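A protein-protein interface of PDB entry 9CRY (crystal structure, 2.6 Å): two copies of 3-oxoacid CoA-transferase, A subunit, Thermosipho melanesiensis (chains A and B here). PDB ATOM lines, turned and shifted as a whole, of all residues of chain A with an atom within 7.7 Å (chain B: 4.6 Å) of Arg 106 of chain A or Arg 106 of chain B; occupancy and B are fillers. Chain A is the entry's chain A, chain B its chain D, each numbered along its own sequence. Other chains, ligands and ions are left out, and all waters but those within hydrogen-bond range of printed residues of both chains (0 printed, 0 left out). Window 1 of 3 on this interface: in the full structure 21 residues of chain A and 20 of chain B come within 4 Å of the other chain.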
ATOM      1  N   MET A  20      15.605 -28.442  10.090  1.00  0.00           N
ATOM      2  CA  MET A  20      15.959 -29.197   8.885  1.00  0.00           C
ATOM      3  C   MET A  20      15.621 -30.673   9.077  1.00  0.00           C
ATOM      4  O   MET A  20      16.018 -31.285  10.076  1.00  0.00           O
ATOM      5  CB  MET A  20      17.445 -29.014   8.624  1.00  0.00           C
ATOM      6  CG  MET A  20      17.759 -27.794   7.826  1.00  0.00           C
ATOM      7  SD  MET A  20      19.505 -27.534   7.902  1.00  0.00           S
ATOM      8  CE  MET A  20      19.641 -25.790   7.559  1.00  0.00           C
ATOM      9  N   GLY A  99      18.045 -28.075  -6.450  1.00  0.00           N
ATOM     10  CA  GLY A  99      19.486 -27.928  -6.430  1.00  0.00           C
ATOM     11  C   GLY A  99      19.954 -26.680  -5.716  1.00  0.00           C
ATOM     12  O   GLY A  99      21.055 -26.658  -5.154  1.00  0.00           O
ATOM     13  N   THR A 100      19.161 -25.607  -5.767  1.00  0.00           N
ATOM     14  CA  THR A 100      19.491 -24.411  -4.998  1.00  0.00           C
ATOM     15  C   THR A 100      19.358 -24.669  -3.507  1.00  0.00           C
ATOM     16  O   THR A 100      20.187 -24.213  -2.708  1.00  0.00           O
ATOM     17  CB  THR A 100      18.598 -23.259  -5.441  1.00  0.00           C
ATOM     18  OG1 THR A 100      18.686 -23.139  -6.859  1.00  0.00           O
ATOM     19  CG2 THR A 100      19.014 -21.960  -4.808  1.00  0.00           C
ATOM     20  N   LEU A 101      18.342 -25.431  -3.118  1.00  0.00           N
ATOM     21  CA  LEU A 101      18.180 -25.760  -1.708  1.00  0.00           C
ATOM     22  C   LEU A 101      19.341 -26.607  -1.222  1.00  0.00           C
ATOM     23  O   LEU A 101      19.830 -26.413  -0.105  1.00  0.00           O
ATOM     24  CB  LEU A 101      16.869 -26.504  -1.493  1.00  0.00           C
ATOM     25  CG  LEU A 101      16.392 -26.765  -0.070  1.00  0.00           C
ATOM     26  CD1 LEU A 101      15.733 -25.540   0.516  1.00  0.00           C
ATOM     27  CD2 LEU A 101      15.445 -27.947  -0.171  1.00  0.00           C
ATOM     28  N   ALA A 102      19.790 -27.565  -2.046  1.00  0.00           N
ATOM     29  CA  ALA A 102      20.937 -28.381  -1.673  1.00  0.00           C
ATOM     30  C   ALA A 102      22.153 -27.510  -1.422  1.00  0.00           C
ATOM     31  O   ALA A 102      22.915 -27.747  -0.481  1.00  0.00           O
ATOM     32  CB  ALA A 102      21.233 -29.409  -2.759  1.00  0.00           C
ATOM     33  N   GLU A 103      22.376 -26.519  -2.276  1.00  0.00           N
ATOM     34  CA  GLU A 103      23.570 -25.698  -2.128  1.00  0.00           C
ATOM     35  C   GLU A 103      23.397 -24.598  -1.086  1.00  0.00           C
ATOM     36  O   GLU A 103      24.391 -24.130  -0.522  1.00  0.00           O
ATOM     37  CB  GLU A 103      23.964 -25.090  -3.474  1.00  0.00           C
ATOM     38  CG  GLU A 103      24.465 -26.083  -4.498  1.00  0.00           C
ATOM     39  CD  GLU A 103      25.827 -26.663  -4.152  1.00  0.00           C
ATOM     40  OE1 GLU A 103      26.770 -25.894  -3.886  1.00  0.00           O
ATOM     41  OE2 GLU A 103      25.962 -27.898  -4.149  1.00  0.00           O
ATOM     42  N   ARG A 104      22.169 -24.142  -0.842  1.00  0.00           N
ATOM     43  CA  ARG A 104      21.967 -23.134   0.195  1.00  0.00           C
ATOM     44  C   ARG A 104      22.208 -23.732   1.572  1.00  0.00           C
ATOM     45  O   ARG A 104      22.939 -23.166   2.394  1.00  0.00           O
ATOM     46  CB  ARG A 104      20.558 -22.552   0.096  1.00  0.00           C
ATOM     47  CG  ARG A 104      20.386 -21.595  -1.054  1.00  0.00           C
ATOM     48  CD  ARG A 104      18.950 -21.136  -1.154  1.00  0.00           C
ATOM     49  NE  ARG A 104      18.630 -20.180  -0.101  1.00  0.00           N
ATOM     50  CZ  ARG A 104      17.407 -19.754   0.191  1.00  0.00           C
ATOM     51  NH1 ARG A 104      16.339 -20.192  -0.466  1.00  0.00           N
ATOM     52  NH2 ARG A 104      17.249 -18.871   1.174  1.00  0.00           N
ATOM     53  N   ILE A 105      21.616 -24.895   1.823  1.00  0.00           N
ATOM     54  CA  ILE A 105      21.884 -25.624   3.051  1.00  0.00           C
ATOM     55  C   ILE A 105      23.375 -25.909   3.165  1.00  0.00           C
ATOM     56  O   ILE A 105      24.000 -25.651   4.202  1.00  0.00           O
ATOM     57  CB  ILE A 105      21.044 -26.910   3.073  1.00  0.00           C
ATOM     58  CG1 ILE A 105      19.556 -26.544   3.094  1.00  0.00           C
ATOM     59  CG2 ILE A 105      21.385 -27.755   4.271  1.00  0.00           C
ATOM     60  CD1 ILE A 105      18.630 -27.733   3.011  1.00  0.00           C
ATOM     61  N   ARG A 106      23.969 -26.448   2.097  1.00  0.00           N
ATOM     62  CA  ARG A 106      25.405 -26.703   2.115  1.00  0.00           C
ATOM     63  C   ARG A 106      26.193 -25.440   2.458  1.00  0.00           C
ATOM     64  O   ARG A 106      27.126 -25.479   3.271  1.00  0.00           O
ATOM     65  CB  ARG A 106      25.859 -27.281   0.775  1.00  0.00           C
ATOM     66  CG  ARG A 106      27.345 -27.558   0.750  1.00  0.00           C
ATOM     67  CD  ARG A 106      27.867 -28.061  -0.600  1.00  0.00           C
ATOM     68  NE  ARG A 106      29.278 -28.415  -0.510  1.00  0.00           N
ATOM     69  CZ  ARG A 106      30.270 -27.538  -0.581  1.00  0.00           C
ATOM     70  NH1 ARG A 106      30.042 -26.252  -0.785  1.00  0.00           N
ATOM     71  NH2 ARG A 106      31.522 -27.963  -0.446  1.00  0.00           N
ATOM     72  N   ALA A 107      25.835 -24.306   1.861  1.00  0.00           N
ATOM     73  CA  ALA A 107      26.559 -23.076   2.153  1.00  0.00           C
ATOM     74  C   ALA A 107      26.600 -22.772   3.650  1.00  0.00           C
ATOM     75  O   ALA A 107      27.639 -22.359   4.183  1.00  0.00           O
ATOM     76  CB  ALA A 107      25.929 -21.911   1.399  1.00  0.00           C
ATOM     77  N   ALA A 108      25.480 -22.966   4.344  1.00  0.00           N
ATOM     78  CA  ALA A 108      25.465 -22.800   5.792  1.00  0.00           C
ATOM     79  C   ALA A 108      26.405 -23.788   6.470  1.00  0.00           C
ATOM     80  O   ALA A 108      27.209 -23.413   7.329  1.00  0.00           O
ATOM     81  CB  ALA A 108      24.040 -22.964   6.316  1.00  0.00           C
ATOM     82  N   GLY A 109      26.354 -25.054   6.055  1.00  0.00           N
ATOM     83  CA  GLY A 109      27.136 -26.065   6.728  1.00  0.00           C
ATOM     84  C   GLY A 109      28.624 -25.908   6.546  1.00  0.00           C
ATOM     85  O   GLY A 109      29.390 -26.224   7.461  1.00  0.00           O
ATOM     86  N   VAL A 110      29.062 -25.370   5.408  1.00  0.00           N
ATOM     87  CA  VAL A 110      30.491 -25.275   5.118  1.00  0.00           C
ATOM     88  C   VAL A 110      31.001 -23.851   5.218  1.00  0.00           C
ATOM     89  O   VAL A 110      32.194 -23.615   4.973  1.00  0.00           O
ATOM     90  CB  VAL A 110      30.838 -25.867   3.734  1.00  0.00           C
ATOM     91  CG1 VAL A 110      30.298 -27.297   3.611  1.00  0.00           C
ATOM     92  CG2 VAL A 110      30.335 -24.991   2.607  1.00  0.00           C
ATOM     93  N   GLY A 111      30.151 -22.897   5.604  1.00  0.00           N
ATOM     94  CA  GLY A 111      30.599 -21.591   6.057  1.00  0.00           C
ATOM     95  C   GLY A 111      30.776 -20.582   4.942  1.00  0.00           C
ATOM     96  O   GLY A 111      31.671 -19.735   5.011  1.00  0.00           O
ATOM     97  N   LEU A 112      29.891 -20.636   3.945  1.00  0.00           N
ATOM     98  CA  LEU A 112      29.896 -19.738   2.803  1.00  0.00           C
ATOM     99  C   LEU A 112      28.812 -18.691   3.023  1.00  0.00           C
ATOM    100  O   LEU A 112      27.759 -18.981   3.593  1.00  0.00           O
ATOM    101  CB  LEU A 112      29.622 -20.496   1.495  1.00  0.00           C
ATOM    102  CG  LEU A 112      30.617 -21.572   1.033  1.00  0.00           C
ATOM    103  CD1 LEU A 112      30.131 -22.322  -0.207  1.00  0.00           C
ATOM    104  CD2 LEU A 112      31.990 -20.969   0.776  1.00  0.00           C
ATOM    105  N   ILE A 115      26.062 -18.590  -2.598  1.00  0.00           N
ATOM    106  CA  ILE A 115      26.492 -19.217  -3.832  1.00  0.00           C
ATOM    107  C   ILE A 115      25.763 -18.531  -4.970  1.00  0.00           C
ATOM    108  O   ILE A 115      24.666 -18.000  -4.785  1.00  0.00           O
ATOM    109  CB  ILE A 115      26.191 -20.727  -3.764  1.00  0.00           C
ATOM    110  CG1 ILE A 115      24.680 -20.893  -3.625  1.00  0.00           C
ATOM    111  CG2 ILE A 115      26.896 -21.354  -2.609  1.00  0.00           C
ATOM    112  CD1 ILE A 115      24.131 -22.146  -4.109  1.00  0.00           C
ATOM    113  N   PRO A 144      22.679 -18.633   2.394  1.00  0.00           N
ATOM    114  CA  PRO A 144      22.694 -19.773   3.323  1.00  0.00           C
ATOM    115  C   PRO A 144      21.408 -19.917   4.120  1.00  0.00           C
ATOM    116  O   PRO A 144      20.832 -18.939   4.607  1.00  0.00           O
ATOM    117  CB  PRO A 144      23.886 -19.465   4.234  1.00  0.00           C
ATOM    118  CG  PRO A 144      24.763 -18.527   3.421  1.00  0.00           C
ATOM    119  CD  PRO A 144      23.802 -17.706   2.611  1.00  0.00           C
ATOM    120  N   ILE A 145      20.970 -21.163   4.257  1.00  0.00           N
ATOM    121  CA  ILE A 145      19.824 -21.522   5.080  1.00  0.00           C
ATOM    122  C   ILE A 145      20.343 -22.161   6.362  1.00  0.00           C
ATOM    123  O   ILE A 145      20.980 -23.216   6.313  1.00  0.00           O
ATOM    124  CB  ILE A 145      18.892 -22.482   4.325  1.00  0.00           C
ATOM    125  CG1 ILE A 145      18.375 -21.812   3.049  1.00  0.00           C
ATOM    126  CG2 ILE A 145      17.736 -22.928   5.213  1.00  0.00           C
ATOM    127  CD1 ILE A 145      17.361 -22.649   2.298  1.00  0.00           C
ATOM    128  N   PHE A 172      19.242 -35.611   1.312  1.00  0.00           N
ATOM    129  CA  PHE A 172      19.584 -34.358   1.978  1.00  0.00           C
ATOM    130  C   PHE A 172      20.193 -34.537   3.371  1.00  0.00           C
ATOM    131  O   PHE A 172      20.705 -33.562   3.935  1.00  0.00           O
ATOM    132  CB  PHE A 172      18.337 -33.458   2.089  1.00  0.00           C
ATOM    133  CG  PHE A 172      18.118 -32.566   0.910  1.00  0.00           C
ATOM    134  CD1 PHE A 172      17.375 -33.004  -0.180  1.00  0.00           C
ATOM    135  CD2 PHE A 172      18.641 -31.290   0.889  1.00  0.00           C
ATOM    136  CE1 PHE A 172      17.169 -32.192  -1.262  1.00  0.00           C
ATOM    137  CE2 PHE A 172      18.436 -30.473  -0.194  1.00  0.00           C
ATOM    138  CZ  PHE A 172      17.701 -30.917  -1.267  1.00  0.00           C
ATOM    139  N   ILE A 175      23.861 -33.368   4.322  1.00  0.00           N
ATOM    140  CA  ILE A 175      24.055 -31.941   4.090  1.00  0.00           C
ATOM    141  C   ILE A 175      23.476 -31.122   5.239  1.00  0.00           C
ATOM    142  O   ILE A 175      24.094 -30.168   5.724  1.00  0.00           O
ATOM    143  CB  ILE A 175      23.390 -31.559   2.757  1.00  0.00           C
ATOM    144  CG1 ILE A 175      24.050 -32.226   1.561  1.00  0.00           C
ATOM    145  CG2 ILE A 175      23.400 -30.039   2.632  1.00  0.00           C
ATOM    146  CD1 ILE A 175      23.089 -32.150   0.335  1.00  0.00           C
ATOM    147  N   MET A 176      22.273 -31.495   5.661  1.00  0.00           N
ATOM    148  CA  MET A 176      21.632 -30.925   6.835  1.00  0.00           C
ATOM    149  C   MET A 176      22.428 -31.155   8.104  1.00  0.00           C
ATOM    150  O   MET A 176      22.555 -30.251   8.939  1.00  0.00           O
ATOM    151  CB  MET A 176      20.243 -31.518   6.943  1.00  0.00           C
ATOM    152  CG  MET A 176      19.337 -31.048   5.864  1.00  0.00           C
ATOM    153  SD  MET A 176      17.873 -31.984   5.836  1.00  0.00           S
ATOM    154  CE  MET A 176      16.712 -30.868   5.023  1.00  0.00           C
ATOM    155  N   LEU A 178      25.381 -30.879   8.592  1.00  0.00           N
ATOM    156  CA  LEU A 178      26.461 -29.918   8.715  1.00  0.00           C
ATOM    157  C   LEU A 178      25.973 -28.492   8.933  1.00  0.00           C
ATOM    158  O   LEU A 178      26.772 -27.631   9.315  1.00  0.00           O
ATOM    159  CB  LEU A 178      27.316 -29.969   7.454  1.00  0.00           C
ATOM    160  CG  LEU A 178      28.436 -30.984   7.266  1.00  0.00           C
ATOM    161  CD1 LEU A 178      28.726 -31.138   5.787  1.00  0.00           C
ATOM    162  CD2 LEU A 178      29.662 -30.506   8.020  1.00  0.00           C
ATOM    163  N   ALA A 179      24.698 -28.219   8.662  1.00  0.00           N
ATOM    164  CA  ALA A 179      24.166 -26.864   8.641  1.00  0.00           C
ATOM    165  C   ALA A 179      23.460 -26.455   9.927  1.00  0.00           C
ATOM    166  O   ALA A 179      23.430 -25.273  10.251  1.00  0.00           O
ATOM    167  CB  ALA A 179      23.193 -26.689   7.469  1.00  0.00           C
ATOM    168  N   ALA B 102      39.494 -25.210  -2.965  1.00  0.00           N
ATOM    169  CA  ALA B 102      38.565 -26.336  -3.031  1.00  0.00           C
ATOM    170  C   ALA B 102      37.203 -25.884  -3.538  1.00  0.00           C
ATOM    171  O   ALA B 102      36.617 -26.510  -4.430  1.00  0.00           O
ATOM    172  CB  ALA B 102      38.422 -26.992  -1.648  1.00  0.00           C
ATOM    173  N   GLU B 103      36.694 -24.777  -3.000  1.00  0.00           N
ATOM    174  CA  GLU B 103      35.343 -24.371  -3.364  1.00  0.00           C
ATOM    175  C   GLU B 103      35.307 -23.679  -4.724  1.00  0.00           C
ATOM    176  O   GLU B 103      34.284 -23.727  -5.410  1.00  0.00           O
ATOM    177  CB  GLU B 103      34.747 -23.454  -2.291  1.00  0.00           C
ATOM    178  CG  GLU B 103      34.494 -24.077  -0.942  1.00  0.00           C
ATOM    179  CD  GLU B 103      33.330 -25.060  -0.961  1.00  0.00           C
ATOM    180  OE1 GLU B 103      32.280 -24.731  -1.565  1.00  0.00           O
ATOM    181  OE2 GLU B 103      33.453 -26.135  -0.328  1.00  0.00           O
ATOM    182  N   ARG B 104      36.393 -23.023  -5.123  1.00  0.00           N
ATOM    183  CA  ARG B 104      36.446 -22.417  -6.449  1.00  0.00           C
ATOM    184  C   ARG B 104      36.424 -23.492  -7.523  1.00  0.00           C
ATOM    185  O   ARG B 104      35.718 -23.371  -8.531  1.00  0.00           O
ATOM    186  CB  ARG B 104      37.681 -21.534  -6.576  1.00  0.00           C
ATOM    187  CG  ARG B 104      37.410 -20.129  -6.096  1.00  0.00           C
ATOM    188  CD  ARG B 104      38.621 -19.247  -6.185  1.00  0.00           C
ATOM    189  NE  ARG B 104      38.788 -18.803  -7.559  1.00  0.00           N
ATOM    190  CZ  ARG B 104      39.926 -18.384  -8.093  1.00  0.00           C
ATOM    191  NH1 ARG B 104      41.046 -18.317  -7.384  1.00  0.00           N
ATOM    192  NH2 ARG B 104      39.942 -18.043  -9.378  1.00  0.00           N
ATOM    193  N   ILE B 105      37.224 -24.543  -7.331  1.00  0.00           N
ATOM    194  CA  ILE B 105      37.212 -25.668  -8.253  1.00  0.00           C
ATOM    195  C   ILE B 105      35.863 -26.366  -8.216  1.00  0.00           C
ATOM    196  O   ILE B 105      35.266 -26.663  -9.259  1.00  0.00           O
ATOM    197  CB  ILE B 105      38.356 -26.645  -7.934  1.00  0.00           C
ATOM    198  CG1 ILE B 105      39.705 -25.981  -8.201  1.00  0.00           C
ATOM    199  CG2 ILE B 105      38.172 -27.908  -8.753  1.00  0.00           C
ATOM    200  CD1 ILE B 105      40.888 -26.698  -7.615  1.00  0.00           C
ATOM    201  N   ARG B 106      35.375 -26.662  -7.010  1.00  0.00           N
ATOM    202  CA  ARG B 106      34.064 -27.283  -6.876  1.00  0.00           C
ATOM    203  C   ARG B 106      32.999 -26.501  -7.634  1.00  0.00           C
ATOM    204  O   ARG B 106      32.145 -27.090  -8.308  1.00  0.00           O
ATOM    205  CB  ARG B 106      33.687 -27.414  -5.401  1.00  0.00           C
ATOM    206  CG  ARG B 106      32.268 -27.890  -5.223  1.00  0.00           C
ATOM    207  CD  ARG B 106      31.873 -28.139  -3.789  1.00  0.00           C
ATOM    208  NE  ARG B 106      30.588 -28.831  -3.738  1.00  0.00           N
ATOM    209  CZ  ARG B 106      29.409 -28.227  -3.838  1.00  0.00           C
ATOM    210  NH1 ARG B 106      29.311 -26.911  -3.945  1.00  0.00           N
ATOM    211  NH2 ARG B 106      28.302 -28.962  -3.839  1.00  0.00           N
ATOM    212  N   ALA B 107      33.015 -25.172  -7.517  1.00  0.00           N
ATOM    213  CA  ALA B 107      31.982 -24.375  -8.168  1.00  0.00           C
ATOM    214  C   ALA B 107      31.973 -24.603  -9.673  1.00  0.00           C
ATOM    215  O   ALA B 107      30.908 -24.726 -10.288  1.00  0.00           O
ATOM    216  CB  ALA B 107      32.197 -22.898  -7.865  1.00  0.00           C
ATOM    217  N   ALA B 108      33.152 -24.655 -10.289  1.00  0.00           N
ATOM    218  CA  ALA B 108      33.214 -25.011 -11.701  1.00  0.00           C
ATOM    219  C   ALA B 108      32.591 -26.380 -11.940  1.00  0.00           C
ATOM    220  O   ALA B 108      31.794 -26.557 -12.868  1.00  0.00           O
ATOM    221  CB  ALA B 108      34.663 -24.960 -12.183  1.00  0.00           C
ATOM    222  N   GLY B 109      32.910 -27.346 -11.074  1.00  0.00           N
ATOM    223  CA  GLY B 109      32.496 -28.722 -11.287  1.00  0.00           C
ATOM    224  C   GLY B 109      31.016 -28.956 -11.109  1.00  0.00           C
ATOM    225  O   GLY B 109      30.459 -29.884 -11.711  1.00  0.00           O
ATOM    226  N   VAL B 110      30.365 -28.165 -10.253  1.00  0.00           N
ATOM    227  CA  VAL B 110      28.945 -28.353  -9.961  1.00  0.00           C
ATOM    228  C   VAL B 110      28.089 -27.280 -10.588  1.00  0.00           C
ATOM    229  O   VAL B 110      26.860 -27.284 -10.380  1.00  0.00           O
ATOM    230  CB  VAL B 110      28.650 -28.419  -8.446  1.00  0.00           C
ATOM    231  CG1 VAL B 110      29.466 -29.496  -7.769  1.00  0.00           C
ATOM    232  CG2 VAL B 110      28.846 -27.052  -7.739  1.00  0.00           C
ATOM    233  N   LEU B 112      28.355 -23.620 -10.529  1.00  0.00           N
ATOM    234  CA  LEU B 112      28.028 -22.398  -9.810  1.00  0.00           C
ATOM    235  C   LEU B 112      28.803 -21.249 -10.436  1.00  0.00           C
ATOM    236  O   LEU B 112      29.924 -21.427 -10.920  1.00  0.00           O
ATOM    237  CB  LEU B 112      28.376 -22.526  -8.319  1.00  0.00           C
ATOM    238  CG  LEU B 112      27.538 -23.562  -7.554  1.00  0.00           C
ATOM    239  CD1 LEU B 112      28.170 -23.867  -6.200  1.00  0.00           C
ATOM    240  CD2 LEU B 112      26.109 -23.120  -7.344  1.00  0.00           C
ATOM    241  N   ILE B 175      37.308 -33.677  -6.576  1.00  0.00           N
ATOM    242  CA  ILE B 175      36.758 -32.362  -6.864  1.00  0.00           C
ATOM    243  C   ILE B 175      37.141 -31.929  -8.266  1.00  0.00           C
ATOM    244  O   ILE B 175      36.316 -31.444  -9.046  1.00  0.00           O
ATOM    245  CB  ILE B 175      37.295 -31.351  -5.839  1.00  0.00           C
ATOM    246  CG1 ILE B 175      36.946 -31.708  -4.395  1.00  0.00           C
ATOM    247  CG2 ILE B 175      36.751 -29.976  -6.118  1.00  0.00           C
ATOM    248  CD1 ILE B 175      37.854 -30.998  -3.369  1.00  0.00           C
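Glu 103 of chain A touches Arg 106 of chain B, and with the chains exchanged Arg 106 of chain A touches Glu 103 of chain B.
Glu 103 of chain A touches Leu 112 of chain B, and with the chains exchanged Leu 112 of chain A touches Glu 103 of chain B.
Arg 106 of chain A touches its own counterpart, Arg 106 of chain B.
Of the 6 pairs that touch across the chains among the printed residues, 5 have their exchanged pair printed and touching as well.
The backbone carbonyl oxygen (O) of Ala 107 of chain A lies within hydrogen-bond range of the backbone NH (N) of Leu 112 of chain A (2.8 Å).
The backbone carbonyl oxygen (O) of Ala 107 of chain B lies within hydrogen-bond range of the backbone NH (N) of Leu 112 of chain B (2.8 Å).
OE2 of Glu 103 of chain A lies within salt-bridge range of NH2 of Arg 106 of chain B (2.6 Å).
The side-chain carboxylate (OE2) of Glu 103 of chain B lies within salt-bridge range of the guanidinium group (NH2) of Arg 106 of chain A (2.7 Å).
The guanidinium group (NH1) of Arg 106 of chain A sits close to the guanidinium group (NH1) of Arg 106 of chain B (3.3 Å).
Printed residues of chain A that touch a printed residue of chain B: Glu 103, Arg 106, Leu 112 and Ile 115.
Hydrophobic or aromatic side chains of chain B within 4 Å of the printed part of chain A: Leu 112.
Along chain B the printed residues that touch a printed residue of chain A span positions 103 to 112.
Of chain B, only Glu 103 and Arg 106 come within 4 Å of Arg 106 of chain A.
Of chain A, only Glu 103 and Arg 106 come within 4 Å of Arg 106 of chain B.
Of the printed residues of chain B, Leu 112 of chain A touches Glu 103 (3.5 Å).
Of the printed residues of chain B, Glu 103 of chain A touches Arg 106 (2.6 Å) and Leu 112 (3.4 Å).
Of the printed residues of chain B, Ile 115 of chain A touches Leu 112.
Printed residues of chain A within 4 Å of Leu 112 of chain B: Glu 103 (3.4 Å) and Ile 115 (3.9 Å).
Printed residues of chain A within 4 Å of Glu 103 of chain B: Arg 106 and Leu 112.
Among the printed residues, pairs that only touch across the chains: Glu 103 of chain A with Leu 112 of chain B (3.4 Å), Leu 112 of chain A with Glu 103 of chain B (3.5 Å) and Ile 115 of chain A with Leu 112 of chain B (3.9 Å).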
